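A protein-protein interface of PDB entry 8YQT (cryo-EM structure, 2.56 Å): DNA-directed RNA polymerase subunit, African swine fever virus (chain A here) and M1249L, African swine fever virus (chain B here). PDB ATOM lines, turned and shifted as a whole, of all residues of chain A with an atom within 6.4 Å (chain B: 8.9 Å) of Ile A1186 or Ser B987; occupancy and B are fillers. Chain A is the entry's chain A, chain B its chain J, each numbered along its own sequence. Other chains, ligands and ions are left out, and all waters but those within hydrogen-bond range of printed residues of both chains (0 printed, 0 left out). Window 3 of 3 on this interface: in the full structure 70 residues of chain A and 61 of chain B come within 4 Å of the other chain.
The guanidinium group (NH1) of Arg B989 is in hydrogen-bond range of the side-chain sulfur (SD) of Met A690 (3.7 Å).
The backbone carbonyl oxygen (O) of Leu A1187 is in hydrogen-bond range of the guanidinium group (NH2) of Arg B936.
The backbone NH (N) of Gly B941 lies close to the side-chain hydroxyl (OG) of Ser A1189, at 3.4 Å.
The side-chain amide oxygen (OD1) of Asn A1181 lies close to the backbone NH (N) of Thr A1183.
O of Phe B932 sits close to NH1 of Arg B936 (3.4 Å).
OH of Tyr B933 sits at hydrogen-bond distance from OE1 of Glu B984 (2.6 Å).
O of Ser B987 sits at hydrogen-bond distance from OG of Ser B990 (2.8 Å).
Among the printed residues, merely in contact across the chains: Met A690 with Phe B932, Met A690 with Lys B985, Thr A1183 with Ser B987, Thr A1183 with Ile B988, Ile A1186 with Arg B936, Ile A1186 with Glu B984, Ile A1186 with Ser B987, Ile A1186 with Ile B988, Leu A1187 with Ile B988, Ser A1189 with Arg B936 and Ser A1189 with Cys B937.
Ile A1186 touches four residues of chain B.
Of chain A, only Thr A1183 and Ile A1186 come within 4 Å of Ser B987.
Printed residues of chain A within 4 Å of Arg B936: Ile A1186 (3.9 Å), Leu A1187 (2.7 Å) and Ser A1189 (3.5 Å).
Printed residues of chain A within 4 Å of Ile B988: Thr A1183, Ile A1186 and Leu A1187.
Printed residues of chain A within 4 Å of Glu B984: Ile A1186.
Leu B942 touches none of the printed residues of chain A.
The nearest residue of chain A that does not touch Ser B987 is Ser A1217 (4.5 Å).
The nearest printed residue of chain A that does not touch Arg B936 is Lys A1188 (4.6 Å).
Of the 20 printed residues of chain B, 9 touch a printed residue of chain A.
Printed residues of chain B that touch a printed residue of chain A: Phe B932, Arg B936, Cys B937, Gly B941, Glu B984, Lys B985, Ser B987, Ile B988 and Arg B989.
Hydrophobic or aromatic side chains of chain B within 4 Å of the printed part of chain A: Phe B932 and Ile B988.
Among the printed residues, no Asp or Glu carboxylate lies within 4 Å of a Lys or Arg side-chain nitrogen of the other chain.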
ATOM      1  N   MET A 690       3.394   8.418 -15.799  1.00  0.00           N
ATOM      2  CA  MET A 690       3.521   7.190 -15.032  1.00  0.00           C
ATOM      3  C   MET A 690       2.756   7.345 -13.727  1.00  0.00           C
ATOM      4  O   MET A 690       3.118   8.202 -12.903  1.00  0.00           O
ATOM      5  CB  MET A 690       4.989   6.866 -14.760  1.00  0.00           C
ATOM      6  CG  MET A 690       5.814   6.663 -16.013  1.00  0.00           C
ATOM      7  SD  MET A 690       5.634   5.001 -16.680  1.00  0.00           S
ATOM      8  CE  MET A 690       7.139   4.237 -16.091  1.00  0.00           C
ATOM      9  N   ASN A1181       0.267 -10.653 -15.391  1.00  0.00           N
ATOM     10  CA  ASN A1181       0.179  -9.353 -16.044  1.00  0.00           C
ATOM     11  C   ASN A1181       1.435  -8.560 -15.712  1.00  0.00           C
ATOM     12  O   ASN A1181       1.587  -8.067 -14.590  1.00  0.00           O
ATOM     13  CB  ASN A1181      -1.077  -8.615 -15.589  1.00  0.00           C
ATOM     14  CG  ASN A1181      -1.376  -7.397 -16.432  1.00  0.00           C
ATOM     15  OD1 ASN A1181      -0.615  -7.044 -17.329  1.00  0.00           O
ATOM     16  ND2 ASN A1181      -2.496  -6.749 -16.150  1.00  0.00           N
ATOM     17  N   LYS A1182       2.342  -8.438 -16.685  1.00  0.00           N
ATOM     18  CA  LYS A1182       3.632  -7.811 -16.416  1.00  0.00           C
ATOM     19  C   LYS A1182       3.495  -6.322 -16.127  1.00  0.00           C
ATOM     20  O   LYS A1182       4.335  -5.753 -15.422  1.00  0.00           O
ATOM     21  CB  LYS A1182       4.584  -8.042 -17.588  1.00  0.00           C
ATOM     22  CG  LYS A1182       5.039  -9.483 -17.730  1.00  0.00           C
ATOM     23  CD  LYS A1182       6.287  -9.596 -18.588  1.00  0.00           C
ATOM     24  CE  LYS A1182       5.972  -9.366 -20.054  1.00  0.00           C
ATOM     25  NZ  LYS A1182       7.164  -9.575 -20.911  1.00  0.00           N
ATOM     26  N   THR A1183       2.462  -5.674 -16.664  1.00  0.00           N
ATOM     27  CA  THR A1183       2.253  -4.260 -16.374  1.00  0.00           C
ATOM     28  C   THR A1183       1.903  -4.043 -14.908  1.00  0.00           C
ATOM     29  O   THR A1183       2.425  -3.122 -14.270  1.00  0.00           O
ATOM     30  CB  THR A1183       1.161  -3.694 -17.281  1.00  0.00           C
ATOM     31  OG1 THR A1183       1.525  -3.896 -18.650  1.00  0.00           O
ATOM     32  CG2 THR A1183       0.973  -2.207 -17.029  1.00  0.00           C
ATOM     33  N   THR A1184       1.026  -4.884 -14.352  1.00  0.00           N
ATOM     34  CA  THR A1184       0.667  -4.760 -12.942  1.00  0.00           C
ATOM     35  C   THR A1184       1.847  -5.082 -12.034  1.00  0.00           C
ATOM     36  O   THR A1184       2.020  -4.439 -10.994  1.00  0.00           O
ATOM     37  CB  THR A1184      -0.521  -5.665 -12.619  1.00  0.00           C
ATOM     38  OG1 THR A1184      -1.622  -5.327 -13.471  1.00  0.00           O
ATOM     39  CG2 THR A1184      -0.953  -5.488 -11.178  1.00  0.00           C
ATOM     40  N   MET A1185       2.667  -6.065 -12.408  1.00  0.00           N
ATOM     41  CA  MET A1185       3.869  -6.364 -11.640  1.00  0.00           C
ATOM     42  C   MET A1185       4.844  -5.195 -11.641  1.00  0.00           C
ATOM     43  O   MET A1185       5.634  -5.048 -10.702  1.00  0.00           O
ATOM     44  CB  MET A1185       4.546  -7.614 -12.197  1.00  0.00           C
ATOM     45  CG  MET A1185       3.805  -8.909 -11.920  1.00  0.00           C
ATOM     46  SD  MET A1185       4.567 -10.298 -12.771  1.00  0.00           S
ATOM     47  CE  MET A1185       6.120 -10.431 -11.893  1.00  0.00           C
ATOM     48  N   ILE A1186       4.813  -4.364 -12.678  1.00  0.00           N
ATOM     49  CA  ILE A1186       5.678  -3.189 -12.747  1.00  0.00           C
ATOM     50  C   ILE A1186       5.047  -1.991 -12.051  1.00  0.00           C
ATOM     51  O   ILE A1186       5.704  -1.309 -11.262  1.00  0.00           O
ATOM     52  CB  ILE A1186       6.016  -2.874 -14.219  1.00  0.00           C
ATOM     53  CG1 ILE A1186       7.008  -3.895 -14.774  1.00  0.00           C
ATOM     54  CG2 ILE A1186       6.563  -1.466 -14.355  1.00  0.00           C
ATOM     55  CD1 ILE A1186       7.297  -3.719 -16.246  1.00  0.00           C
ATOM     56  N   LEU A1187       3.769  -1.721 -12.324  1.00  0.00           N
ATOM     57  CA  LEU A1187       3.103  -0.572 -11.718  1.00  0.00           C
ATOM     58  C   LEU A1187       3.010  -0.698 -10.205  1.00  0.00           C
ATOM     59  O   LEU A1187       3.126   0.308  -9.495  1.00  0.00           O
ATOM     60  CB  LEU A1187       1.709  -0.396 -12.315  1.00  0.00           C
ATOM     61  CG  LEU A1187       1.608   0.205 -13.717  1.00  0.00           C
ATOM     62  CD1 LEU A1187       0.153   0.338 -14.112  1.00  0.00           C
ATOM     63  CD2 LEU A1187       2.304   1.553 -13.789  1.00  0.00           C
ATOM     64  N   LYS A1188       2.783  -1.905  -9.693  1.00  0.00           N
ATOM     65  CA  LYS A1188       2.722  -2.136  -8.255  1.00  0.00           C
ATOM     66  C   LYS A1188       4.066  -2.511  -7.653  1.00  0.00           C
ATOM     67  O   LYS A1188       4.156  -2.647  -6.429  1.00  0.00           O
ATOM     68  CB  LYS A1188       1.700  -3.230  -7.935  1.00  0.00           C
ATOM     69  CG  LYS A1188       0.315  -2.944  -8.472  1.00  0.00           C
ATOM     70  CD  LYS A1188      -0.310  -1.745  -7.796  1.00  0.00           C
ATOM     71  CE  LYS A1188      -1.682  -1.460  -8.365  1.00  0.00           C
ATOM     72  NZ  LYS A1188      -2.291  -0.234  -7.779  1.00  0.00           N
ATOM     73  N   SER A1189       5.100  -2.688  -8.476  1.00  0.00           N
ATOM     74  CA  SER A1189       6.447  -3.037  -8.026  1.00  0.00           C
ATOM     75  C   SER A1189       6.426  -4.321  -7.191  1.00  0.00           C
ATOM     76  O   SER A1189       6.769  -4.344  -6.009  1.00  0.00           O
ATOM     77  CB  SER A1189       7.082  -1.885  -7.242  1.00  0.00           C
ATOM     78  OG  SER A1189       8.407  -2.214  -6.876  1.00  0.00           O
ATOM     79  N   ILE A1190       6.012  -5.395  -7.850  1.00  0.00           N
ATOM     80  CA  ILE A1190       5.865  -6.699  -7.218  1.00  0.00           C
ATOM     81  C   ILE A1190       6.806  -7.667  -7.913  1.00  0.00           C
ATOM     82  O   ILE A1190       6.700  -7.883  -9.126  1.00  0.00           O
ATOM     83  CB  ILE A1190       4.414  -7.197  -7.275  1.00  0.00           C
ATOM     84  CG1 ILE A1190       3.548  -6.347  -6.351  1.00  0.00           C
ATOM     85  CG2 ILE A1190       4.336  -8.654  -6.882  1.00  0.00           C
ATOM     86  CD1 ILE A1190       2.093  -6.653  -6.434  1.00  0.00           C
ATOM     87  N   SER A1217       9.931  -7.902 -23.715  1.00  0.00           N
ATOM     88  CA  SER A1217       8.512  -7.907 -24.043  1.00  0.00           C
ATOM     89  C   SER A1217       8.187  -9.042 -25.004  1.00  0.00           C
ATOM     90  O   SER A1217       8.984  -9.385 -25.882  1.00  0.00           O
ATOM     91  CB  SER A1217       8.103  -6.569 -24.658  1.00  0.00           C
ATOM     92  OG  SER A1217       8.201  -5.517 -23.715  1.00  0.00           O
ATOM     93  N   PHE B 932       8.439   8.055 -10.138  1.00  0.00           N
ATOM     94  CA  PHE B 932       8.249   6.620 -10.308  1.00  0.00           C
ATOM     95  C   PHE B 932       8.999   5.840  -9.233  1.00  0.00           C
ATOM     96  O   PHE B 932       8.412   5.016  -8.525  1.00  0.00           O
ATOM     97  CB  PHE B 932       8.702   6.184 -11.703  1.00  0.00           C
ATOM     98  CG  PHE B 932       8.321   4.773 -12.045  1.00  0.00           C
ATOM     99  CD1 PHE B 932       7.025   4.462 -12.411  1.00  0.00           C
ATOM    100  CD2 PHE B 932       9.257   3.755 -11.983  1.00  0.00           C
ATOM    101  CE1 PHE B 932       6.673   3.166 -12.716  1.00  0.00           C
ATOM    102  CE2 PHE B 932       8.909   2.460 -12.289  1.00  0.00           C
ATOM    103  CZ  PHE B 932       7.617   2.165 -12.656  1.00  0.00           C
ATOM    104  N   TYR B 933      10.295   6.096  -9.093  1.00  0.00           N
ATOM    105  CA  TYR B 933      11.133   5.364  -8.145  1.00  0.00           C
ATOM    106  C   TYR B 933      11.194   6.052  -6.786  1.00  0.00           C
ATOM    107  O   TYR B 933      12.269   6.268  -6.234  1.00  0.00           O
ATOM    108  CB  TYR B 933      12.531   5.191  -8.725  1.00  0.00           C
ATOM    109  CG  TYR B 933      12.649   4.082  -9.743  1.00  0.00           C
ATOM    110  CD1 TYR B 933      11.866   2.942  -9.647  1.00  0.00           C
ATOM    111  CD2 TYR B 933      13.538   4.178 -10.803  1.00  0.00           C
ATOM    112  CE1 TYR B 933      11.968   1.929 -10.573  1.00  0.00           C
ATOM    113  CE2 TYR B 933      13.649   3.168 -11.734  1.00  0.00           C
ATOM    114  CZ  TYR B 933      12.861   2.046 -11.615  1.00  0.00           C
ATOM    115  OH  TYR B 933      12.964   1.035 -12.542  1.00  0.00           O
ATOM    116  N   SER B 935       8.522   5.053  -4.229  1.00  0.00           N
ATOM    117  CA  SER B 935       8.185   3.829  -3.517  1.00  0.00           C
ATOM    118  C   SER B 935       8.610   2.589  -4.279  1.00  0.00           C
ATOM    119  O   SER B 935       9.009   1.601  -3.665  1.00  0.00           O
ATOM    120  CB  SER B 935       6.681   3.764  -3.244  1.00  0.00           C
ATOM    121  OG  SER B 935       6.271   4.805  -2.378  1.00  0.00           O
ATOM    122  N   ARG B 936       8.522   2.624  -5.608  1.00  0.00           N
ATOM    123  CA  ARG B 936       9.073   1.569  -6.444  1.00  0.00           C
ATOM    124  C   ARG B 936      10.547   1.389  -6.142  1.00  0.00           C
ATOM    125  O   ARG B 936      11.303   2.361  -6.099  1.00  0.00           O
ATOM    126  CB  ARG B 936       8.897   1.920  -7.923  1.00  0.00           C
ATOM    127  CG  ARG B 936       7.691   1.330  -8.616  1.00  0.00           C
ATOM    128  CD  ARG B 936       6.429   1.923  -8.075  1.00  0.00           C
ATOM    129  NE  ARG B 936       5.324   1.867  -9.022  1.00  0.00           N
ATOM    130  CZ  ARG B 936       4.802   2.929  -9.618  1.00  0.00           C
ATOM    131  NH1 ARG B 936       5.288   4.140  -9.416  1.00  0.00           N
ATOM    132  NH2 ARG B 936       3.759   2.773 -10.426  1.00  0.00           N
ATOM    133  N   CYS B 937      10.949   0.173  -5.935  1.00  0.00           N
ATOM    134  CA  CYS B 937      12.387  -0.021  -5.858  1.00  0.00           C
ATOM    135  C   CYS B 937      12.889  -0.619  -7.166  1.00  0.00           C
ATOM    136  O   CYS B 937      12.313  -1.602  -7.648  1.00  0.00           O
ATOM    137  CB  CYS B 937      12.756  -0.927  -4.693  1.00  0.00           C
ATOM    138  SG  CYS B 937      14.517  -0.935  -4.285  1.00  0.00           S
ATOM    139  N   GLY B 940      13.298  -4.242  -7.174  1.00  0.00           N
ATOM    140  CA  GLY B 940      12.097  -5.013  -6.899  1.00  0.00           C
ATOM    141  C   GLY B 940      11.455  -4.636  -5.581  1.00  0.00           C
ATOM    142  O   GLY B 940      12.110  -4.229  -4.624  1.00  0.00           O
ATOM    143  N   GLY B 941      10.134  -4.784  -5.533  1.00  0.00           N
ATOM    144  CA  GLY B 941       9.416  -4.466  -4.317  1.00  0.00           C
ATOM    145  C   GLY B 941       9.428  -2.978  -4.019  1.00  0.00           C
ATOM    146  O   GLY B 941       9.493  -2.131  -4.913  1.00  0.00           O
ATOM    147  N   LEU B 942       9.364  -2.659  -2.733  1.00  0.00           N
ATOM    148  CA  LEU B 942       9.404  -1.286  -2.253  1.00  0.00           C
ATOM    149  C   LEU B 942      10.733  -1.022  -1.557  1.00  0.00           C
ATOM    150  O   LEU B 942      11.472  -1.945  -1.206  1.00  0.00           O
ATOM    151  CB  LEU B 942       8.228  -1.009  -1.311  1.00  0.00           C
ATOM    152  CG  LEU B 942       6.858  -1.397  -1.869  1.00  0.00           C
ATOM    153  CD1 LEU B 942       5.761  -1.129  -0.859  1.00  0.00           C
ATOM    154  CD2 LEU B 942       6.585  -0.655  -3.161  1.00  0.00           C
ATOM    155  N   GLN B 980      16.805   0.150 -17.433  1.00  0.00           N
ATOM    156  CA  GLN B 980      15.669  -0.614 -16.941  1.00  0.00           C
ATOM    157  C   GLN B 980      14.454   0.292 -16.857  1.00  0.00           C
ATOM    158  O   GLN B 980      13.354  -0.101 -17.242  1.00  0.00           O
ATOM    159  CB  GLN B 980      15.989  -1.241 -15.583  1.00  0.00           C
ATOM    160  CG  GLN B 980      14.985  -0.930 -14.487  1.00  0.00           C
ATOM    161  CD  GLN B 980      15.527   0.061 -13.478  1.00  0.00           C
ATOM    162  OE1 GLN B 980      15.317   1.267 -13.605  1.00  0.00           O
ATOM    163  NE2 GLN B 980      16.227  -0.441 -12.470  1.00  0.00           N
ATOM    164  N   TYR B 981      14.650   1.512 -16.368  1.00  0.00           N
ATOM    165  CA  TYR B 981      13.549   2.462 -16.313  1.00  0.00           C
ATOM    166  C   TYR B 981      12.967   2.606 -17.704  1.00  0.00           C
ATOM    167  O   TYR B 981      11.750   2.682 -17.869  1.00  0.00           O
ATOM    168  CB  TYR B 981      14.027   3.815 -15.795  1.00  0.00           C
ATOM    169  CG  TYR B 981      12.910   4.779 -15.464  1.00  0.00           C
ATOM    170  CD1 TYR B 981      12.225   4.690 -14.260  1.00  0.00           C
ATOM    171  CD2 TYR B 981      12.543   5.778 -16.353  1.00  0.00           C
ATOM    172  CE1 TYR B 981      11.207   5.570 -13.952  1.00  0.00           C
ATOM    173  CE2 TYR B 981      11.525   6.663 -16.054  1.00  0.00           C
ATOM    174  CZ  TYR B 981      10.860   6.553 -14.852  1.00  0.00           C
ATOM    175  OH  TYR B 981       9.844   7.431 -14.549  1.00  0.00           O
ATOM    176  N   ASP B 982      13.836   2.636 -18.708  1.00  0.00           N
ATOM    177  CA  ASP B 982      13.372   2.757 -20.087  1.00  0.00           C
ATOM    178  C   ASP B 982      12.557   1.543 -20.514  1.00  0.00           C
ATOM    179  O   ASP B 982      11.495   1.689 -21.130  1.00  0.00           O
ATOM    180  CB  ASP B 982      14.560   2.959 -21.029  1.00  0.00           C
ATOM    181  CG  ASP B 982      15.073   4.381 -21.021  1.00  0.00           C
ATOM    182  OD1 ASP B 982      14.269   5.304 -20.772  1.00  0.00           O
ATOM    183  OD2 ASP B 982      16.279   4.580 -21.272  1.00  0.00           O
ATOM    184  N   LYS B 983      13.039   0.337 -20.205  1.00  0.00           N
ATOM    185  CA  LYS B 983      12.305  -0.867 -20.584  1.00  0.00           C
ATOM    186  C   LYS B 983      10.966  -0.947 -19.866  1.00  0.00           C
ATOM    187  O   LYS B 983       9.947  -1.287 -20.477  1.00  0.00           O
ATOM    188  CB  LYS B 983      13.145  -2.109 -20.295  1.00  0.00           C
ATOM    189  CG  LYS B 983      14.369  -2.248 -21.181  1.00  0.00           C
ATOM    190  CD  LYS B 983      15.064  -3.579 -20.951  1.00  0.00           C
ATOM    191  CE  LYS B 983      16.255  -3.751 -21.878  1.00  0.00           C
ATOM    192  NZ  LYS B 983      17.383  -2.856 -21.500  1.00  0.00           N
ATOM    193  N   GLU B 984      10.946  -0.638 -18.568  1.00  0.00           N
ATOM    194  CA  GLU B 984       9.686  -0.620 -17.835  1.00  0.00           C
ATOM    195  C   GLU B 984       8.743   0.430 -18.402  1.00  0.00           C
ATOM    196  O   GLU B 984       7.542   0.184 -18.542  1.00  0.00           O
ATOM    197  CB  GLU B 984       9.945  -0.368 -16.348  1.00  0.00           C
ATOM    198  CG  GLU B 984      10.768  -1.452 -15.665  1.00  0.00           C
ATOM    199  CD  GLU B 984      10.700  -1.382 -14.150  1.00  0.00           C
ATOM    200  OE1 GLU B 984      11.714  -1.016 -13.521  1.00  0.00           O
ATOM    201  OE2 GLU B 984       9.635  -1.699 -13.583  1.00  0.00           O
ATOM    202  N   LYS B 985       9.277   1.601 -18.757  1.00  0.00           N
ATOM    203  CA  LYS B 985       8.440   2.701 -19.222  1.00  0.00           C
ATOM    204  C   LYS B 985       7.683   2.331 -20.493  1.00  0.00           C
ATOM    205  O   LYS B 985       6.492   2.635 -20.621  1.00  0.00           O
ATOM    206  CB  LYS B 985       9.303   3.940 -19.450  1.00  0.00           C
ATOM    207  CG  LYS B 985       8.529   5.221 -19.660  1.00  0.00           C
ATOM    208  CD  LYS B 985       9.480   6.378 -19.901  1.00  0.00           C
ATOM    209  CE  LYS B 985       8.722   7.670 -20.097  1.00  0.00           C
ATOM    210  NZ  LYS B 985       8.021   8.059 -18.847  1.00  0.00           N
ATOM    211  N   MET B 986       8.351   1.678 -21.441  1.00  0.00           N
ATOM    212  CA  MET B 986       7.705   1.260 -22.677  1.00  0.00           C
ATOM    213  C   MET B 986       6.940  -0.049 -22.538  1.00  0.00           C
ATOM    214  O   MET B 986       6.178  -0.401 -23.444  1.00  0.00           O
ATOM    215  CB  MET B 986       8.740   1.131 -23.800  1.00  0.00           C
ATOM    216  CG  MET B 986       9.431  -0.217 -23.863  1.00  0.00           C
ATOM    217  SD  MET B 986      11.113  -0.103 -24.504  1.00  0.00           S
ATOM    218  CE  MET B 986      11.296  -1.719 -25.249  1.00  0.00           C
ATOM    219  N   SER B 987       7.121  -0.774 -21.432  1.00  0.00           N
ATOM    220  CA  SER B 987       6.353  -1.990 -21.199  1.00  0.00           C
ATOM    221  C   SER B 987       4.911  -1.692 -20.806  1.00  0.00           C
ATOM    222  O   SER B 987       3.998  -2.398 -21.248  1.00  0.00           O
ATOM    223  CB  SER B 987       7.022  -2.840 -20.122  1.00  0.00           C
ATOM    224  OG  SER B 987       6.280  -4.020 -19.878  1.00  0.00           O
ATOM    225  N   ILE B 988       4.684  -0.674 -19.974  1.00  0.00           N
ATOM    226  CA  ILE B 988       3.316  -0.261 -19.673  1.00  0.00           C
ATOM    227  C   ILE B 988       2.639   0.276 -20.925  1.00  0.00           C
ATOM    228  O   ILE B 988       1.473  -0.031 -21.204  1.00  0.00           O
ATOM    229  CB  ILE B 988       3.287   0.779 -18.537  1.00  0.00           C
ATOM    230  CG1 ILE B 988       3.774   0.179 -17.221  1.00  0.00           C
ATOM    231  CG2 ILE B 988       1.888   1.342 -18.364  1.00  0.00           C
ATOM    232  CD1 ILE B 988       5.129   0.646 -16.813  1.00  0.00           C
ATOM    233  N   ARG B 989       3.361   1.082 -21.703  1.00  0.00           N
ATOM    234  CA  ARG B 989       2.802   1.783 -22.852  1.00  0.00           C
ATOM    235  C   ARG B 989       2.692   0.906 -24.093  1.00  0.00           C
ATOM    236  O   ARG B 989       2.530   1.439 -25.198  1.00  0.00           O
ATOM    237  CB  ARG B 989       3.644   3.023 -23.165  1.00  0.00           C
ATOM    238  CG  ARG B 989       3.625   4.087 -22.078  1.00  0.00           C
ATOM    239  CD  ARG B 989       2.274   4.786 -21.990  1.00  0.00           C
ATOM    240  NE  ARG B 989       1.561   4.508 -20.748  1.00  0.00           N
ATOM    241  CZ  ARG B 989       1.974   4.864 -19.538  1.00  0.00           C
ATOM    242  NH1 ARG B 989       3.101   5.532 -19.356  1.00  0.00           N
ATOM    243  NH2 ARG B 989       1.230   4.547 -18.481  1.00  0.00           N
ATOM    244  N   SER B 990       2.778  -0.410 -23.948  1.00  0.00           N
ATOM    245  CA  SER B 990       2.681  -1.339 -25.063  1.00  0.00           C
ATOM    246  C   SER B 990       1.355  -2.092 -25.000  1.00  0.00           C
ATOM    247  O   SER B 990       0.540  -1.886 -24.096  1.00  0.00           O
ATOM    248  CB  SER B 990       3.869  -2.306 -25.060  1.00  0.00           C
ATOM    249  OG  SER B 990       3.803  -3.194 -23.959  1.00  0.00           O
ATOM    250  N   ILE B 991       1.153  -2.969 -25.980  1.00  0.00           N
ATOM    251  CA  ILE B 991      -0.060  -3.777 -26.109  1.00  0.00           C
ATOM    252  C   ILE B 991      -1.298  -2.886 -26.182  1.00  0.00           C
ATOM    253  O   ILE B 991      -1.972  -2.652 -25.180  1.00  0.00           O
ATOM    254  CB  ILE B 991      -0.182  -4.799 -24.958  1.00  0.00           C
ATOM    255  CG1 ILE B 991       1.123  -5.583 -24.804  1.00  0.00           C
ATOM    256  CG2 ILE B 991      -1.334  -5.762 -25.211  1.00  0.00           C
ATOM    257  CD1 ILE B 991       1.154  -6.477 -23.586  1.00  0.00           C
